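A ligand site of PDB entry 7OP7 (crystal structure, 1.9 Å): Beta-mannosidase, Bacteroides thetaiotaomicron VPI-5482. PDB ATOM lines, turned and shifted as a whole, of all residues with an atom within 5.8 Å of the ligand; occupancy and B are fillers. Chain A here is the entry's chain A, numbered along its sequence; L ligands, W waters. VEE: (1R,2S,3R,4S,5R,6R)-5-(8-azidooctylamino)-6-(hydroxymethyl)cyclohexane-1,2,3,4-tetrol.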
ATOM      1  N   ASN A 155      10.082 -14.493 -14.970  1.00  0.00           N
ATOM      2  CA  ASN A 155       8.997 -15.235 -14.251  1.00  0.00           C
ATOM      3  C   ASN A 155       9.355 -15.443 -12.782  1.00  0.00           C
ATOM      4  O   ASN A 155       8.504 -15.995 -12.006  1.00  0.00           O
ATOM      5  CB  ASN A 155       8.604 -16.545 -14.920  1.00  0.00           C
ATOM      6  CG  ASN A 155       7.780 -16.294 -16.181  1.00  0.00           C
ATOM      7  OD1 ASN A 155       6.577 -16.091 -16.112  1.00  0.00           O
ATOM      8  ND2 ASN A 155       8.456 -16.243 -17.302  1.00  0.00           N
ATOM      9  N   TRP A 175       5.462 -17.548 -11.914  1.00  0.00           N
ATOM     10  CA  TRP A 175       5.315 -17.669 -13.381  1.00  0.00           C
ATOM     11  C   TRP A 175       4.063 -16.918 -13.813  1.00  0.00           C
ATOM     12  O   TRP A 175       3.210 -16.668 -12.933  1.00  0.00           O
ATOM     13  CB  TRP A 175       5.206 -19.173 -13.766  1.00  0.00           C
ATOM     14  CG  TRP A 175       5.878 -19.424 -15.071  1.00  0.00           C
ATOM     15  CD1 TRP A 175       5.331 -19.393 -16.318  1.00  0.00           C
ATOM     16  CD2 TRP A 175       7.279 -19.628 -15.241  1.00  0.00           C
ATOM     17  NE1 TRP A 175       6.298 -19.545 -17.273  1.00  0.00           N
ATOM     18  CE2 TRP A 175       7.515 -19.695 -16.632  1.00  0.00           C
ATOM     19  CE3 TRP A 175       8.359 -19.757 -14.356  1.00  0.00           C
ATOM     20  CZ2 TRP A 175       8.787 -19.906 -17.157  1.00  0.00           C
ATOM     21  CZ3 TRP A 175       9.614 -19.977 -14.887  1.00  0.00           C
ATOM     22  CH2 TRP A 175       9.818 -20.014 -16.265  1.00  0.00           C
ATOM     23  N   ASP A 176       3.890 -16.711 -15.120  1.00  0.00           N
ATOM     24  CA  ASP A 176       2.781 -15.908 -15.716  1.00  0.00           C
ATOM     25  C   ASP A 176       1.401 -16.643 -15.594  1.00  0.00           C
ATOM     26  O   ASP A 176       0.423 -16.016 -16.012  1.00  0.00           O
ATOM     27  CB  ASP A 176       3.127 -15.438 -17.132  1.00  0.00           C
ATOM     28  CG  ASP A 176       3.210 -16.554 -18.173  1.00  0.00           C
ATOM     29  OD1 ASP A 176       2.952 -17.757 -17.830  1.00  0.00           O
ATOM     30  OD2 ASP A 176       3.576 -16.247 -19.272  1.00  0.00           O
ATOM     31  N   TRP A 177       1.291 -17.779 -14.867  1.00  0.00           N
ATOM     32  CA  TRP A 177       0.028 -18.415 -14.392  1.00  0.00           C
ATOM     33  C   TRP A 177       0.202 -18.900 -12.953  1.00  0.00           C
ATOM     34  O   TRP A 177      -0.643 -19.664 -12.431  1.00  0.00           O
ATOM     35  CB  TRP A 177      -0.347 -19.600 -15.323  1.00  0.00           C
ATOM     36  CG  TRP A 177       0.841 -20.359 -15.812  1.00  0.00           C
ATOM     37  CD1 TRP A 177       1.432 -20.287 -17.038  1.00  0.00           C
ATOM     38  CD2 TRP A 177       1.678 -21.215 -15.016  1.00  0.00           C
ATOM     39  NE1 TRP A 177       2.537 -21.092 -17.083  1.00  0.00           N
ATOM     40  CE2 TRP A 177       2.716 -21.663 -15.849  1.00  0.00           C
ATOM     41  CE3 TRP A 177       1.616 -21.654 -13.691  1.00  0.00           C
ATOM     42  CZ2 TRP A 177       3.727 -22.507 -15.393  1.00  0.00           C
ATOM     43  CZ3 TRP A 177       2.624 -22.476 -13.225  1.00  0.00           C
ATOM     44  CH2 TRP A 177       3.650 -22.890 -14.077  1.00  0.00           C
ATOM     45  N   TRP A 372       6.839 -29.598 -19.478  1.00  0.00           N
ATOM     46  CA  TRP A 372       7.548 -28.313 -19.747  1.00  0.00           C
ATOM     47  C   TRP A 372       8.613 -28.038 -18.681  1.00  0.00           C
ATOM     48  O   TRP A 372       8.456 -28.492 -17.513  1.00  0.00           O
ATOM     49  CB  TRP A 372       6.478 -27.228 -19.765  1.00  0.00           C
ATOM     50  CG  TRP A 372       6.939 -25.840 -19.545  1.00  0.00           C
ATOM     51  CD1 TRP A 372       7.318 -24.911 -20.471  1.00  0.00           C
ATOM     52  CD2 TRP A 372       6.845 -25.157 -18.298  1.00  0.00           C
ATOM     53  NE1 TRP A 372       7.586 -23.708 -19.856  1.00  0.00           N
ATOM     54  CE2 TRP A 372       7.291 -23.824 -18.532  1.00  0.00           C
ATOM     55  CE3 TRP A 372       6.503 -25.555 -17.017  1.00  0.00           C
ATOM     56  CZ2 TRP A 372       7.352 -22.886 -17.531  1.00  0.00           C
ATOM     57  CZ3 TRP A 372       6.592 -24.625 -16.018  1.00  0.00           C
ATOM     58  CH2 TRP A 372       6.983 -23.297 -16.287  1.00  0.00           C
ATOM     59  N   CYS A 401      13.217 -20.256 -20.124  1.00  0.00           N
ATOM     60  CA  CYS A 401      12.879 -18.827 -20.385  1.00  0.00           C
ATOM     61  C   CYS A 401      13.952 -17.813 -19.944  1.00  0.00           C
ATOM     62  O   CYS A 401      13.697 -16.588 -20.014  1.00  0.00           O
ATOM     63  CB  CYS A 401      11.598 -18.515 -19.668  1.00  0.00           C
ATOM     64  SG  CYS A 401      10.143 -19.206 -20.483  1.00  0.00           S
ATOM     65  N   ASN A 438      12.990 -24.870 -22.488  1.00  0.00           N
ATOM     66  CA  ASN A 438      11.876 -24.071 -23.027  1.00  0.00           C
ATOM     67  C   ASN A 438      12.372 -22.666 -23.348  1.00  0.00           C
ATOM     68  O   ASN A 438      12.576 -21.890 -22.414  1.00  0.00           O
ATOM     69  CB  ASN A 438      10.706 -24.015 -22.048  1.00  0.00           C
ATOM     70  CG  ASN A 438       9.530 -23.286 -22.679  1.00  0.00           C
ATOM     71  OD1 ASN A 438       8.864 -23.851 -23.553  1.00  0.00           O
ATOM     72  ND2 ASN A 438       9.362 -22.004 -22.344  1.00  0.00           N
ATOM     73  N   GLU A 439      12.533 -22.352 -24.626  1.00  0.00           N
ATOM     74  CA  GLU A 439      12.606 -20.983 -25.220  1.00  0.00           C
ATOM     75  C   GLU A 439      13.837 -20.206 -24.767  1.00  0.00           C
ATOM     76  O   GLU A 439      13.853 -18.972 -24.963  1.00  0.00           O
ATOM     77  CB  GLU A 439      11.360 -20.161 -24.874  1.00  0.00           C
ATOM     78  CG  GLU A 439      10.065 -20.671 -25.422  1.00  0.00           C
ATOM     79  CD  GLU A 439       8.806 -20.035 -24.838  1.00  0.00           C
ATOM     80  OE1 GLU A 439       8.872 -19.420 -23.757  1.00  0.00           O
ATOM     81  OE2 GLU A 439       7.711 -20.225 -25.404  1.00  0.00           O
ATOM     82  N   TRP A 447      14.015 -11.897 -27.361  1.00  0.00           N
ATOM     83  CA  TRP A 447      13.286 -11.134 -26.323  1.00  0.00           C
ATOM     84  C   TRP A 447      14.074  -9.885 -26.013  1.00  0.00           C
ATOM     85  O   TRP A 447      13.768  -9.219 -25.032  1.00  0.00           O
ATOM     86  CB  TRP A 447      13.046 -11.982 -25.086  1.00  0.00           C
ATOM     87  CG  TRP A 447      12.173 -13.165 -25.390  1.00  0.00           C
ATOM     88  CD1 TRP A 447      11.711 -13.540 -26.627  1.00  0.00           C
ATOM     89  CD2 TRP A 447      11.706 -14.134 -24.454  1.00  0.00           C
ATOM     90  NE1 TRP A 447      10.963 -14.687 -26.499  1.00  0.00           N
ATOM     91  CE2 TRP A 447      10.941 -15.073 -25.171  1.00  0.00           C
ATOM     92  CE3 TRP A 447      11.832 -14.280 -23.066  1.00  0.00           C
ATOM     93  CZ2 TRP A 447      10.309 -16.136 -24.553  1.00  0.00           C
ATOM     94  CZ3 TRP A 447      11.228 -15.352 -22.451  1.00  0.00           C
ATOM     95  CH2 TRP A 447      10.465 -16.256 -23.191  1.00  0.00           C
ATOM     96  N   TRP A 496       8.108 -17.051 -34.103  1.00  0.00           N
ATOM     97  CA  TRP A 496       6.728 -16.615 -34.456  1.00  0.00           C
ATOM     98  C   TRP A 496       6.773 -15.347 -35.309  1.00  0.00           C
ATOM     99  O   TRP A 496       5.952 -15.292 -36.256  1.00  0.00           O
ATOM    100  CB  TRP A 496       5.820 -16.449 -33.228  1.00  0.00           C
ATOM    101  CG  TRP A 496       6.127 -15.300 -32.318  1.00  0.00           C
ATOM    102  CD1 TRP A 496       7.138 -15.217 -31.422  1.00  0.00           C
ATOM    103  CD2 TRP A 496       5.391 -14.070 -32.219  1.00  0.00           C
ATOM    104  NE1 TRP A 496       7.104 -14.010 -30.795  1.00  0.00           N
ATOM    105  CE2 TRP A 496       6.049 -13.279 -31.258  1.00  0.00           C
ATOM    106  CE3 TRP A 496       4.292 -13.531 -32.886  1.00  0.00           C
ATOM    107  CZ2 TRP A 496       5.614 -12.006 -30.920  1.00  0.00           C
ATOM    108  CZ3 TRP A 496       3.852 -12.278 -32.538  1.00  0.00           C
ATOM    109  CH2 TRP A 496       4.490 -11.532 -31.545  1.00  0.00           C
ATOM    110  N   HIS A 508       6.604 -22.216 -31.473  1.00  0.00           N
ATOM    111  CA  HIS A 508       5.719 -21.669 -30.404  1.00  0.00           C
ATOM    112  C   HIS A 508       4.986 -20.475 -30.987  1.00  0.00           C
ATOM    113  O   HIS A 508       5.593 -19.426 -31.172  1.00  0.00           O
ATOM    114  CB  HIS A 508       6.500 -21.209 -29.160  1.00  0.00           C
ATOM    115  CG  HIS A 508       7.132 -22.312 -28.416  1.00  0.00           C
ATOM    116  ND1 HIS A 508       7.534 -22.168 -27.085  1.00  0.00           N
ATOM    117  CD2 HIS A 508       7.505 -23.544 -28.813  1.00  0.00           C
ATOM    118  CE1 HIS A 508       8.083 -23.302 -26.689  1.00  0.00           C
ATOM    119  NE2 HIS A 508       8.083 -24.181 -27.718  1.00  0.00           N
ATOM    120  N   TRP A 510       3.222 -17.252 -30.819  1.00  0.00           N
ATOM    121  CA  TRP A 510       2.788 -16.179 -29.896  1.00  0.00           C
ATOM    122  C   TRP A 510       1.988 -15.126 -30.695  1.00  0.00           C
ATOM    123  O   TRP A 510       1.577 -14.157 -30.078  1.00  0.00           O
ATOM    124  CB  TRP A 510       4.008 -15.605 -29.149  1.00  0.00           C
ATOM    125  N   TRP A 513      -2.810 -14.518 -28.955  1.00  0.00           N
ATOM    126  CA  TRP A 513      -2.563 -13.992 -27.596  1.00  0.00           C
ATOM    127  C   TRP A 513      -1.581 -12.807 -27.670  1.00  0.00           C
ATOM    128  O   TRP A 513      -2.063 -11.740 -27.870  1.00  0.00           O
ATOM    129  CB  TRP A 513      -2.151 -15.080 -26.592  1.00  0.00           C
ATOM    130  CG  TRP A 513      -2.194 -14.569 -25.186  1.00  0.00           C
ATOM    131  CD1 TRP A 513      -1.105 -14.203 -24.452  1.00  0.00           C
ATOM    132  CD2 TRP A 513      -3.343 -14.261 -24.358  1.00  0.00           C
ATOM    133  NE1 TRP A 513      -1.484 -13.757 -23.209  1.00  0.00           N
ATOM    134  CE2 TRP A 513      -2.856 -13.752 -23.130  1.00  0.00           C
ATOM    135  CE3 TRP A 513      -4.722 -14.339 -24.524  1.00  0.00           C
ATOM    136  CZ2 TRP A 513      -3.698 -13.325 -22.101  1.00  0.00           C
ATOM    137  CZ3 TRP A 513      -5.554 -13.922 -23.508  1.00  0.00           C
ATOM    138  CH2 TRP A 513      -5.053 -13.445 -22.305  1.00  0.00           C
ATOM    139  N   TYR A 514      -0.272 -12.991 -27.550  1.00  0.00           N
ATOM    140  CA  TYR A 514       0.716 -11.893 -27.388  1.00  0.00           C
ATOM    141  C   TYR A 514       0.609 -10.993 -28.624  1.00  0.00           C
ATOM    142  O   TYR A 514       0.484  -9.834 -28.438  1.00  0.00           O
ATOM    143  CB  TYR A 514       2.178 -12.299 -27.084  1.00  0.00           C
ATOM    144  N   GLU A 532       3.792 -25.181 -28.951  1.00  0.00           N
ATOM    145  CA  GLU A 532       3.136 -24.271 -27.982  1.00  0.00           C
ATOM    146  C   GLU A 532       2.267 -23.274 -28.732  1.00  0.00           C
ATOM    147  O   GLU A 532       2.801 -22.591 -29.656  1.00  0.00           O
ATOM    148  CB  GLU A 532       4.202 -23.584 -27.126  1.00  0.00           C
ATOM    149  CG  GLU A 532       3.605 -22.836 -25.928  1.00  0.00           C
ATOM    150  CD  GLU A 532       4.362 -21.566 -25.555  1.00  0.00           C
ATOM    151  OE1 GLU A 532       4.750 -20.873 -26.519  1.00  0.00           O
ATOM    152  OE2 GLU A 532       4.505 -21.213 -24.315  1.00  0.00           O
ATOM    153  N   SER A 566       0.181 -12.574 -16.504  1.00  0.00           N
ATOM    154  CA  SER A 566       0.651 -12.400 -17.888  1.00  0.00           C
ATOM    155  C   SER A 566       0.869 -10.900 -18.162  1.00  0.00           C
ATOM    156  O   SER A 566       0.321 -10.068 -17.401  1.00  0.00           O
ATOM    157  CB  SER A 566      -0.293 -13.041 -18.833  1.00  0.00           C
ATOM    158  OG  SER A 566      -1.219 -12.116 -19.359  1.00  0.00           O
ATOM    159  N   TRP A 622      -0.941 -24.921 -25.223  1.00  0.00           N
ATOM    160  CA  TRP A 622      -0.517 -24.343 -23.947  1.00  0.00           C
ATOM    161  C   TRP A 622      -1.830 -23.892 -23.325  1.00  0.00           C
ATOM    162  O   TRP A 622      -2.364 -22.970 -23.856  1.00  0.00           O
ATOM    163  CB  TRP A 622       0.504 -23.221 -24.148  1.00  0.00           C
ATOM    164  CG  TRP A 622       0.938 -22.763 -22.779  1.00  0.00           C
ATOM    165  CD1 TRP A 622       0.255 -21.944 -21.905  1.00  0.00           C
ATOM    166  CD2 TRP A 622       1.992 -23.369 -22.009  1.00  0.00           C
ATOM    167  NE1 TRP A 622       0.878 -21.933 -20.676  1.00  0.00           N
ATOM    168  CE2 TRP A 622       1.960 -22.784 -20.720  1.00  0.00           C
ATOM    169  CE3 TRP A 622       3.054 -24.227 -22.345  1.00  0.00           C
ATOM    170  CZ2 TRP A 622       2.917 -23.104 -19.756  1.00  0.00           C
ATOM    171  CZ3 TRP A 622       3.982 -24.564 -21.375  1.00  0.00           C
ATOM    172  CH2 TRP A 622       3.896 -24.032 -20.086  1.00  0.00           C
ATOM    173  N   GLN A 623      -2.364 -24.492 -22.247  1.00  0.00           N
ATOM    174  CA  GLN A 623      -1.725 -25.489 -21.404  1.00  0.00           C
ATOM    175  C   GLN A 623      -2.808 -26.455 -20.904  1.00  0.00           C
ATOM    176  O   GLN A 623      -4.011 -26.088 -20.925  1.00  0.00           O
ATOM    177  CB  GLN A 623      -1.057 -24.841 -20.162  1.00  0.00           C
ATOM    178  CG  GLN A 623      -2.020 -24.230 -19.138  1.00  0.00           C
ATOM    179  CD  GLN A 623      -1.396 -23.123 -18.301  1.00  0.00           C
ATOM    180  OE1 GLN A 623      -1.160 -22.017 -18.746  1.00  0.00           O
ATOM    181  NE2 GLN A 623      -1.175 -23.365 -17.046  1.00  0.00           N
ATOM    182  N   TRP A 633      -4.173 -20.149 -19.366  1.00  0.00           N
ATOM    183  CA  TRP A 633      -4.359 -20.773 -20.683  1.00  0.00           C
ATOM    184  C   TRP A 633      -4.822 -22.218 -20.509  1.00  0.00           C
ATOM    185  O   TRP A 633      -4.948 -22.852 -21.518  1.00  0.00           O
ATOM    186  CB  TRP A 633      -3.075 -20.685 -21.487  1.00  0.00           C
ATOM    187  CG  TRP A 633      -2.508 -19.319 -21.672  1.00  0.00           C
ATOM    188  CD1 TRP A 633      -2.532 -18.586 -22.813  1.00  0.00           C
ATOM    189  CD2 TRP A 633      -1.741 -18.550 -20.718  1.00  0.00           C
ATOM    190  NE1 TRP A 633      -1.897 -17.392 -22.629  1.00  0.00           N
ATOM    191  CE2 TRP A 633      -1.405 -17.341 -21.351  1.00  0.00           C
ATOM    192  CE3 TRP A 633      -1.315 -18.746 -19.408  1.00  0.00           C
ATOM    193  CZ2 TRP A 633      -0.658 -16.337 -20.723  1.00  0.00           C
ATOM    194  CZ3 TRP A 633      -0.562 -17.754 -18.781  1.00  0.00           C
ATOM    195  CH2 TRP A 633      -0.285 -16.546 -19.413  1.00  0.00           C
HETATM  196  C1  VEE L   1       4.975 -20.124 -23.517  1.00  0.00           C
HETATM  197  C2  VEE L   1       6.030 -20.178 -22.420  1.00  0.00           C
HETATM  198  C3  VEE L   1       5.345 -20.618 -21.138  1.00  0.00           C
HETATM  199  C4  VEE L   1       4.335 -19.493 -20.745  1.00  0.00           C
HETATM  200  C5  VEE L   1       3.284 -19.322 -21.866  1.00  0.00           C
HETATM  201  C6  VEE L   1       3.956 -19.015 -23.218  1.00  0.00           C
HETATM  202  C8  VEE L   1       2.188 -18.331 -21.494  1.00  0.00           C
HETATM  203  C14 VEE L   1       4.894 -17.088 -24.569  1.00  0.00           C
HETATM  204  C15 VEE L   1       5.435 -15.667 -24.472  1.00  0.00           C
HETATM  205  C16 VEE L   1       6.395 -15.269 -25.587  1.00  0.00           C
HETATM  206  C17 VEE L   1       6.422 -13.766 -25.897  1.00  0.00           C
HETATM  207  C18 VEE L   1       7.768 -13.119 -25.696  1.00  0.00           C
HETATM  208  N7  VEE L   1       4.513 -17.629 -23.255  1.00  0.00           N
HETATM  209  O9  VEE L   1       2.654 -17.005 -21.665  1.00  0.00           O
HETATM  210  O11 VEE L   1       3.603 -19.722 -19.519  1.00  0.00           O
HETATM  211  O12 VEE L   1       6.411 -20.797 -20.198  1.00  0.00           O
HETATM  212  O13 VEE L   1       6.673 -18.885 -22.173  1.00  0.00           O
HETATM  213  O   HOH W   1       2.346 -14.760 -23.629  1.00  0.00           O
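The side-chain carboxylate (OE2) of Glu 532 is covalently linked to a carbon (C1) of the ligand. OD1 of Asp 176 lies within hydrogen-bond range of O11 of the ligand, at 2.7 Å. An oxygen (O13) of the ligand lies within hydrogen-bond range of the side-chain carboxylate (OE1) of Glu 439, at 2.8 Å. The indole nitrogen of Trp 177 is in hydrogen-bond range of an oxygen (O11) of the ligand. The indole nitrogen (NE1) of Trp 372 lies within hydrogen-bond range of an oxygen (O12) of the ligand (3.2 Å). O12 of the ligand lies within hydrogen-bond range of NE1 of Trp 175.
The indole nitrogen (NE1) of Trp 177 lies close to the side-chain carboxylate (OD1) of Asp 176 (3.4 Å). N of Ser 566 is in hydrogen-bond range of O of Asp 176, at 3.5 Å. The side-chain carboxylate (OE1) of Glu 439 lies within hydrogen-bond range of the side-chain amide nitrogen (ND2) of Asn 438 (3.0 Å). The side-chain sulfur (SG) of Cys 401 is in hydrogen-bond range of the side-chain carboxylate (OE1) of Glu 439 (3.5 Å). The side-chain amide nitrogen (ND2) of Asn 438 lies close to the indole nitrogen (NE1) of Trp 372 (3.5 Å). N of Trp 175 sits at hydrogen-bond distance from O of Asn 155 (3.4 Å). The backbone carbonyl oxygen of Trp 633 lies within hydrogen-bond range of the backbone NH of Gln 623, at 3.1 Å. The backbone carbonyl oxygen (O) of Asn 438 sits at hydrogen-bond distance from the backbone NH (N) of Cys 401 (2.9 Å).
Residues that only touch the ligand: Cys 401 (3.9 Å), Asn 438 (3.8 Å), Trp 447 (3.6 Å), Trp 622 (3.5 Å) and Trp 633 (3.5 Å). Along chain A the residues within 4 Å of the ligand span positions 175 to 633.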
